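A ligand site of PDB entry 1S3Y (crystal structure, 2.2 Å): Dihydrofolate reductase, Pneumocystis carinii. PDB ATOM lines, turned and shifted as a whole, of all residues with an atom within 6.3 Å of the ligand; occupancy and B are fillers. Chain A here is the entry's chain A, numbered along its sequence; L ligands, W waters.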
ATOM      1  N   ILE A  10     -19.931  -5.671 -16.890  1.00  0.00           N
ATOM      2  CA  ILE A  10     -19.454  -5.809 -18.267  1.00  0.00           C
ATOM      3  C   ILE A  10     -18.726  -4.509 -18.518  1.00  0.00           C
ATOM      4  O   ILE A  10     -19.243  -3.437 -18.176  1.00  0.00           O
ATOM      5  CB  ILE A  10     -20.621  -6.054 -19.289  1.00  0.00           C
ATOM      6  CG1 ILE A  10     -20.060  -6.143 -20.706  1.00  0.00           C
ATOM      7  CG2 ILE A  10     -21.650  -4.942 -19.248  1.00  0.00           C
ATOM      8  CD1 ILE A  10     -21.036  -6.771 -21.673  1.00  0.00           C
ATOM      9  N   VAL A  11     -17.525  -4.587 -19.078  1.00  0.00           N
ATOM     10  CA  VAL A  11     -16.708  -3.399 -19.276  1.00  0.00           C
ATOM     11  C   VAL A  11     -15.635  -3.620 -20.341  1.00  0.00           C
ATOM     12  O   VAL A  11     -15.271  -4.755 -20.641  1.00  0.00           O
ATOM     13  CB  VAL A  11     -16.022  -3.028 -17.894  1.00  0.00           C
ATOM     14  CG1 VAL A  11     -15.148  -4.174 -17.423  1.00  0.00           C
ATOM     15  CG2 VAL A  11     -15.206  -1.769 -17.995  1.00  0.00           C
ATOM     16  N   ALA A  12     -15.140  -2.524 -20.907  1.00  0.00           N
ATOM     17  CA  ALA A  12     -14.077  -2.551 -21.911  1.00  0.00           C
ATOM     18  C   ALA A  12     -12.988  -1.678 -21.315  1.00  0.00           C
ATOM     19  O   ALA A  12     -13.251  -0.539 -20.937  1.00  0.00           O
ATOM     20  CB  ALA A  12     -14.579  -1.968 -23.246  1.00  0.00           C
ATOM     21  N   LEU A  25     -13.666   9.124 -25.457  1.00  0.00           N
ATOM     22  CA  LEU A  25     -13.901   7.701 -25.744  1.00  0.00           C
ATOM     23  C   LEU A  25     -12.820   7.263 -26.709  1.00  0.00           C
ATOM     24  O   LEU A  25     -13.091   7.130 -27.906  1.00  0.00           O
ATOM     25  CB  LEU A  25     -15.316   7.479 -26.343  1.00  0.00           C
ATOM     26  CG  LEU A  25     -15.659   6.030 -26.710  1.00  0.00           C
ATOM     27  CD1 LEU A  25     -15.124   5.074 -25.680  1.00  0.00           C
ATOM     28  CD2 LEU A  25     -17.176   5.916 -26.825  1.00  0.00           C
ATOM     29  N   GLU A  32     -17.082  -4.350 -30.995  1.00  0.00           N
ATOM     30  CA  GLU A  32     -17.139  -4.463 -29.550  1.00  0.00           C
ATOM     31  C   GLU A  32     -18.573  -4.197 -29.092  1.00  0.00           C
ATOM     32  O   GLU A  32     -19.162  -4.999 -28.353  1.00  0.00           O
ATOM     33  CB  GLU A  32     -16.146  -3.483 -28.917  1.00  0.00           C
ATOM     34  CG  GLU A  32     -15.532  -3.981 -27.598  1.00  0.00           C
ATOM     35  CD  GLU A  32     -16.541  -4.013 -26.482  1.00  0.00           C
ATOM     36  OE1 GLU A  32     -17.253  -3.006 -26.325  1.00  0.00           O
ATOM     37  OE2 GLU A  32     -16.634  -5.020 -25.756  1.00  0.00           O
ATOM     38  N   ILE A  33     -19.142  -3.092 -29.572  1.00  0.00           N
ATOM     39  CA  ILE A  33     -20.525  -2.696 -29.257  1.00  0.00           C
ATOM     40  C   ILE A  33     -21.469  -3.835 -29.614  1.00  0.00           C
ATOM     41  O   ILE A  33     -22.444  -4.115 -28.908  1.00  0.00           O
ATOM     42  CB  ILE A  33     -20.975  -1.477 -30.068  1.00  0.00           C
ATOM     43  CG1 ILE A  33     -19.898  -0.416 -30.072  1.00  0.00           C
ATOM     44  CG2 ILE A  33     -22.264  -0.918 -29.472  1.00  0.00           C
ATOM     45  CD1 ILE A  33     -19.455   0.044 -28.714  1.00  0.00           C
ATOM     46  N   TYR A  35     -20.784  -6.971 -29.655  1.00  0.00           N
ATOM     47  CA  TYR A  35     -20.641  -8.005 -28.639  1.00  0.00           C
ATOM     48  C   TYR A  35     -21.430  -7.574 -27.407  1.00  0.00           C
ATOM     49  O   TYR A  35     -22.200  -8.342 -26.844  1.00  0.00           O
ATOM     50  CB  TYR A  35     -19.152  -8.157 -28.291  1.00  0.00           C
ATOM     51  CG  TYR A  35     -18.865  -9.089 -27.142  1.00  0.00           C
ATOM     52  CD1 TYR A  35     -18.954 -10.467 -27.300  1.00  0.00           C
ATOM     53  CD2 TYR A  35     -18.477  -8.578 -25.893  1.00  0.00           C
ATOM     54  CE1 TYR A  35     -18.668 -11.329 -26.228  1.00  0.00           C
ATOM     55  CE2 TYR A  35     -18.189  -9.431 -24.824  1.00  0.00           C
ATOM     56  CZ  TYR A  35     -18.288 -10.795 -25.006  1.00  0.00           C
ATOM     57  OH  TYR A  35     -18.046 -11.625 -23.942  1.00  0.00           O
ATOM     58  N   PHE A  36     -21.231  -6.310 -27.016  1.00  0.00           N
ATOM     59  CA  PHE A  36     -21.896  -5.730 -25.856  1.00  0.00           C
ATOM     60  C   PHE A  36     -23.399  -5.920 -25.929  1.00  0.00           C
ATOM     61  O   PHE A  36     -24.006  -6.413 -24.979  1.00  0.00           O
ATOM     62  CB  PHE A  36     -21.594  -4.225 -25.767  1.00  0.00           C
ATOM     63  CG  PHE A  36     -22.450  -3.489 -24.765  1.00  0.00           C
ATOM     64  CD1 PHE A  36     -22.217  -3.622 -23.397  1.00  0.00           C
ATOM     65  CD2 PHE A  36     -23.496  -2.654 -25.185  1.00  0.00           C
ATOM     66  CE1 PHE A  36     -23.013  -2.929 -22.463  1.00  0.00           C
ATOM     67  CE2 PHE A  36     -24.285  -1.967 -24.262  1.00  0.00           C
ATOM     68  CZ  PHE A  36     -24.043  -2.104 -22.897  1.00  0.00           C
ATOM     69  N   THR A  61     -22.820   7.868 -17.761  1.00  0.00           N
ATOM     70  CA  THR A  61     -22.881   6.892 -18.816  1.00  0.00           C
ATOM     71  C   THR A  61     -24.129   7.130 -19.653  1.00  0.00           C
ATOM     72  O   THR A  61     -24.073   7.128 -20.886  1.00  0.00           O
ATOM     73  CB  THR A  61     -22.876   5.465 -18.245  1.00  0.00           C
ATOM     74  OG1 THR A  61     -21.603   5.192 -17.676  1.00  0.00           O
ATOM     75  CG2 THR A  61     -23.184   4.443 -19.334  1.00  0.00           C
ATOM     76  N   SER A  64     -23.500   9.823 -21.949  1.00  0.00           N
ATOM     77  CA  SER A  64     -22.474   9.443 -22.917  1.00  0.00           C
ATOM     78  C   SER A  64     -23.072   8.698 -24.119  1.00  0.00           C
ATOM     79  O   SER A  64     -22.420   8.548 -25.151  1.00  0.00           O
ATOM     80  CB  SER A  64     -21.418   8.564 -22.235  1.00  0.00           C
ATOM     81  OG  SER A  64     -20.408   8.169 -23.140  1.00  0.00           O
ATOM     82  N   ILE A  65     -24.310   8.230 -23.985  1.00  0.00           N
ATOM     83  CA  ILE A  65     -24.956   7.500 -25.068  1.00  0.00           C
ATOM     84  C   ILE A  65     -25.853   8.422 -25.897  1.00  0.00           C
ATOM     85  O   ILE A  65     -26.709   9.119 -25.360  1.00  0.00           O
ATOM     86  CB  ILE A  65     -25.809   6.339 -24.520  1.00  0.00           C
ATOM     87  CG1 ILE A  65     -24.953   5.426 -23.640  1.00  0.00           C
ATOM     88  CG2 ILE A  65     -26.407   5.542 -25.684  1.00  0.00           C
ATOM     89  CD1 ILE A  65     -25.727   4.310 -22.977  1.00  0.00           C
ATOM     90  N   PRO A  66     -25.660   8.433 -27.228  1.00  0.00           N
ATOM     91  CA  PRO A  66     -26.450   9.273 -28.138  1.00  0.00           C
ATOM     92  C   PRO A  66     -27.938   8.963 -28.025  1.00  0.00           C
ATOM     93  O   PRO A  66     -28.332   7.814 -27.809  1.00  0.00           O
ATOM     94  CB  PRO A  66     -25.892   8.894 -29.505  1.00  0.00           C
ATOM     95  CG  PRO A  66     -24.461   8.602 -29.215  1.00  0.00           C
ATOM     96  CD  PRO A  66     -24.561   7.764 -27.952  1.00  0.00           C
ATOM     97  N   PHE A  69     -29.454   5.446 -29.520  1.00  0.00           N
ATOM     98  CA  PHE A  69     -29.605   4.169 -28.844  1.00  0.00           C
ATOM     99  C   PHE A  69     -30.113   4.275 -27.404  1.00  0.00           C
ATOM    100  O   PHE A  69     -29.877   3.370 -26.587  1.00  0.00           O
ATOM    101  CB  PHE A  69     -28.261   3.416 -28.883  1.00  0.00           C
ATOM    102  CG  PHE A  69     -27.565   3.491 -30.216  1.00  0.00           C
ATOM    103  CD1 PHE A  69     -28.104   2.874 -31.334  1.00  0.00           C
ATOM    104  CD2 PHE A  69     -26.372   4.204 -30.350  1.00  0.00           C
ATOM    105  CE1 PHE A  69     -27.478   2.979 -32.580  1.00  0.00           C
ATOM    106  CE2 PHE A  69     -25.734   4.309 -31.589  1.00  0.00           C
ATOM    107  CZ  PHE A  69     -26.292   3.698 -32.703  1.00  0.00           C
ATOM    108  N   LEU A  72     -31.537   1.599 -24.200  1.00  0.00           N
ATOM    109  CA  LEU A  72     -31.143   0.335 -24.804  1.00  0.00           C
ATOM    110  C   LEU A  72     -32.367  -0.550 -24.933  1.00  0.00           C
ATOM    111  O   LEU A  72     -32.890  -1.045 -23.930  1.00  0.00           O
ATOM    112  CB  LEU A  72     -30.077  -0.349 -23.959  1.00  0.00           C
ATOM    113  CG  LEU A  72     -28.838   0.497 -23.669  1.00  0.00           C
ATOM    114  CD1 LEU A  72     -27.922  -0.267 -22.733  1.00  0.00           C
ATOM    115  CD2 LEU A  72     -28.113   0.824 -24.960  1.00  0.00           C
ATOM    116  N   VAL A 122     -24.118  -4.684 -14.933  1.00  0.00           N
ATOM    117  CA  VAL A 122     -23.633  -3.359 -14.502  1.00  0.00           C
ATOM    118  C   VAL A 122     -22.771  -2.996 -15.692  1.00  0.00           C
ATOM    119  O   VAL A 122     -21.731  -3.625 -15.933  1.00  0.00           O
ATOM    120  CB  VAL A 122     -22.723  -3.428 -13.241  1.00  0.00           C
ATOM    121  CG1 VAL A 122     -22.218  -2.037 -12.881  1.00  0.00           C
ATOM    122  CG2 VAL A 122     -23.478  -4.049 -12.099  1.00  0.00           C
ATOM    123  N   ILE A 123     -23.176  -1.989 -16.449  1.00  0.00           N
ATOM    124  CA  ILE A 123     -22.454  -1.644 -17.669  1.00  0.00           C
ATOM    125  C   ILE A 123     -21.649  -0.383 -17.658  1.00  0.00           C
ATOM    126  O   ILE A 123     -20.704  -0.214 -18.441  1.00  0.00           O
ATOM    127  CB  ILE A 123     -23.435  -1.539 -18.856  1.00  0.00           C
ATOM    128  CG1 ILE A 123     -24.376  -0.338 -18.672  1.00  0.00           C
ATOM    129  CG2 ILE A 123     -24.262  -2.766 -18.936  1.00  0.00           C
ATOM    130  CD1 ILE A 123     -25.095   0.122 -19.960  1.00  0.00           C
ATOM    131  N   GLY A 124     -21.990   0.543 -16.777  1.00  0.00           N
ATOM    132  CA  GLY A 124     -21.253   1.764 -16.832  1.00  0.00           C
ATOM    133  C   GLY A 124     -21.177   2.648 -15.633  1.00  0.00           C
ATOM    134  O   GLY A 124     -22.097   2.753 -14.814  1.00  0.00           O
ATOM    135  N   TYR A 129     -19.112   1.124 -10.925  1.00  0.00           N
ATOM    136  CA  TYR A 129     -18.287  -0.060 -10.896  1.00  0.00           C
ATOM    137  C   TYR A 129     -17.730  -0.208  -9.486  1.00  0.00           C
ATOM    138  O   TYR A 129     -17.658  -1.317  -8.960  1.00  0.00           O
ATOM    139  CB  TYR A 129     -17.134   0.046 -11.892  1.00  0.00           C
ATOM    140  CG  TYR A 129     -17.537  -0.158 -13.332  1.00  0.00           C
ATOM    141  CD1 TYR A 129     -18.534  -1.073 -13.691  1.00  0.00           C
ATOM    142  CD2 TYR A 129     -16.886   0.530 -14.346  1.00  0.00           C
ATOM    143  CE1 TYR A 129     -18.881  -1.288 -15.035  1.00  0.00           C
ATOM    144  CE2 TYR A 129     -17.214   0.336 -15.681  1.00  0.00           C
ATOM    145  CZ  TYR A 129     -18.191  -0.565 -16.017  1.00  0.00           C
ATOM    146  OH  TYR A 129     -18.447  -0.736 -17.358  1.00  0.00           O
ATOM    147  N   MET A 142     -17.409  -9.388 -17.296  1.00  0.00           N
ATOM    148  CA  MET A 142     -17.256  -9.635 -18.719  1.00  0.00           C
ATOM    149  C   MET A 142     -16.373  -8.472 -19.102  1.00  0.00           C
ATOM    150  O   MET A 142     -16.805  -7.328 -19.134  1.00  0.00           O
ATOM    151  CB  MET A 142     -18.598  -9.496 -19.476  1.00  0.00           C
ATOM    152  CG  MET A 142     -19.709 -10.372 -18.999  1.00  0.00           C
ATOM    153  SD  MET A 142     -19.252 -12.090 -19.053  1.00  0.00           S
ATOM    154  CE  MET A 142     -19.816 -12.577 -20.673  1.00  0.00           C
ATOM    155  N   ALA A 143     -15.132  -8.785 -19.415  1.00  0.00           N
ATOM    156  CA  ALA A 143     -14.163  -7.744 -19.740  1.00  0.00           C
ATOM    157  C   ALA A 143     -13.646  -7.802 -21.165  1.00  0.00           C
ATOM    158  O   ALA A 143     -13.464  -8.866 -21.718  1.00  0.00           O
ATOM    159  CB  ALA A 143     -13.003  -7.840 -18.771  1.00  0.00           C
ATOM    160  N   THR A 144     -13.410  -6.635 -21.755  1.00  0.00           N
ATOM    161  CA  THR A 144     -12.844  -6.561 -23.094  1.00  0.00           C
ATOM    162  C   THR A 144     -11.501  -5.868 -22.895  1.00  0.00           C
ATOM    163  O   THR A 144     -11.467  -4.713 -22.498  1.00  0.00           O
ATOM    164  CB  THR A 144     -13.710  -5.726 -24.067  1.00  0.00           C
ATOM    165  OG1 THR A 144     -14.921  -6.418 -24.370  1.00  0.00           O
ATOM    166  CG2 THR A 144     -12.923  -5.464 -25.366  1.00  0.00           C
HETATM  167  C1  LIG L   1     -18.223  -3.311 -22.980  1.00  0.00           C
HETATM  168  C2  LIG L   1     -19.514  -1.931 -21.567  1.00  0.00           C
HETATM  169  C3  LIG L   1     -19.721  -0.955 -22.774  1.00  0.00           C
HETATM  170  C4  LIG L   1     -21.116   0.703 -24.127  1.00  0.00           C
HETATM  171  C5  LIG L   1     -19.947   0.773 -25.204  1.00  0.00           C
HETATM  172  C6  LIG L   1     -19.084  -1.351 -23.963  1.00  0.00           C
HETATM  173  C7  LIG L   1     -21.965   2.065 -24.032  1.00  0.00           C
HETATM  174  C8  LIG L   1     -23.500   1.879 -26.196  1.00  0.00           C
HETATM  175  C9  LIG L   1     -21.972   3.738 -25.974  1.00  0.00           C
HETATM  176  C10 LIG L   1     -21.016   4.696 -25.563  1.00  0.00           C
HETATM  177  C11 LIG L   1     -20.751   5.901 -26.543  1.00  0.00           C
HETATM  178  C12 LIG L   1     -21.476   5.945 -27.741  1.00  0.00           C
HETATM  179  C13 LIG L   1     -22.417   4.959 -28.071  1.00  0.00           C
HETATM  180  C14 LIG L   1     -22.653   3.887 -27.185  1.00  0.00           C
HETATM  181  C15 LIG L   1     -23.644   2.791 -27.466  1.00  0.00           C
HETATM  182  N1  LIG L   1     -18.376  -2.509 -23.973  1.00  0.00           N
HETATM  183  N2  LIG L   1     -17.440  -4.524 -23.190  1.00  0.00           N
HETATM  184  N3  LIG L   1     -18.797  -3.031 -21.761  1.00  0.00           N
HETATM  185  N4  LIG L   1     -20.122  -1.615 -20.307  1.00  0.00           N
HETATM  186  C16 LIG L   1     -20.534   0.340 -22.711  1.00  0.00           C
HETATM  187  C17 LIG L   1     -19.107  -0.598 -25.272  1.00  0.00           C
HETATM  188  N5  LIG L   1     -22.491   2.507 -25.348  1.00  0.00           N
HETATM  189  O   HOH W   1     -16.776  -7.590 -22.170  1.00  0.00           O
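O of Ile 123 lies within hydrogen-bond range of OH of Tyr 129, at 2.6 Å. OE2 of Glu 32 is in hydrogen-bond range of OG1 of Thr 144, at 2.6 Å. O of Ile 10 is in hydrogen-bond range of OH of Tyr 129, at 2.9 Å. The backbone NH (N) of Ile 10 sits at hydrogen-bond distance from the backbone carbonyl oxygen (O) of Val 122 (2.9 Å). O of Val 11 is in hydrogen-bond range of N of Thr 144, 2.9 Å away. The backbone carbonyl oxygen (O) of Met 142 is in hydrogen-bond range of the backbone NH (N) of Val 11 (2.8 Å).
Water W1 lies within hydrogen-bond range of the backbone carbonyl oxygen of Met 142 (3.0 Å), the side-chain hydroxyl of Thr 144 (3.1 Å), a nitrogen (N2) of the ligand (3.3 Å) and the backbone NH of Ala 143 (3.4 Å).
N4 of the ligand sits at hydrogen-bond distance from O of Ile 123, 2.4 Å away. OE1 of Glu 32 is in salt-bridge range of N1 of the ligand, 2.7 Å away. A nitrogen (N4) of the ligand lies within hydrogen-bond range of the backbone carbonyl oxygen (O) of Ile 10 (2.9 Å). N of Val 11 lies close to N3 of the ligand (3.4 Å). The backbone carbonyl oxygen (O) of Val 11 is in hydrogen-bond range of a nitrogen (N2) of the ligand. OG1 of Thr 144 lies within hydrogen-bond range of N2 of the ligand.
N of Ala 12 touches N3 of the ligand, 3.8 Å away. Leu 25 touches the ligand. Ile 33 touches the ligand. Phe 36 touches the ligand (CD1 to C2, 3.7 Å). O of Ser 64 touches C11 of the ligand (3.4 Å). Pro 66 touches the ligand (CD to C13, 3.5 Å). Tyr 129 touches the ligand (OH to N4, 3.5 Å). Hydrophobic or aromatic side chains that line the ligand: Ile 10, Ala 12, Leu 25, Ile 33, Phe 36, Pro 66 and Ile 123. 12 residues have an atom within 4 Å of the ligand: Ile 10, Val 11, Ala 12, Leu 25, Glu 32, Ile 33, Phe 36, Ser 64, Pro 66, Ile 123, Tyr 129 and Thr 144. The nearest printed residue that does not touch the ligand is Ile 65 (4.1 Å).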
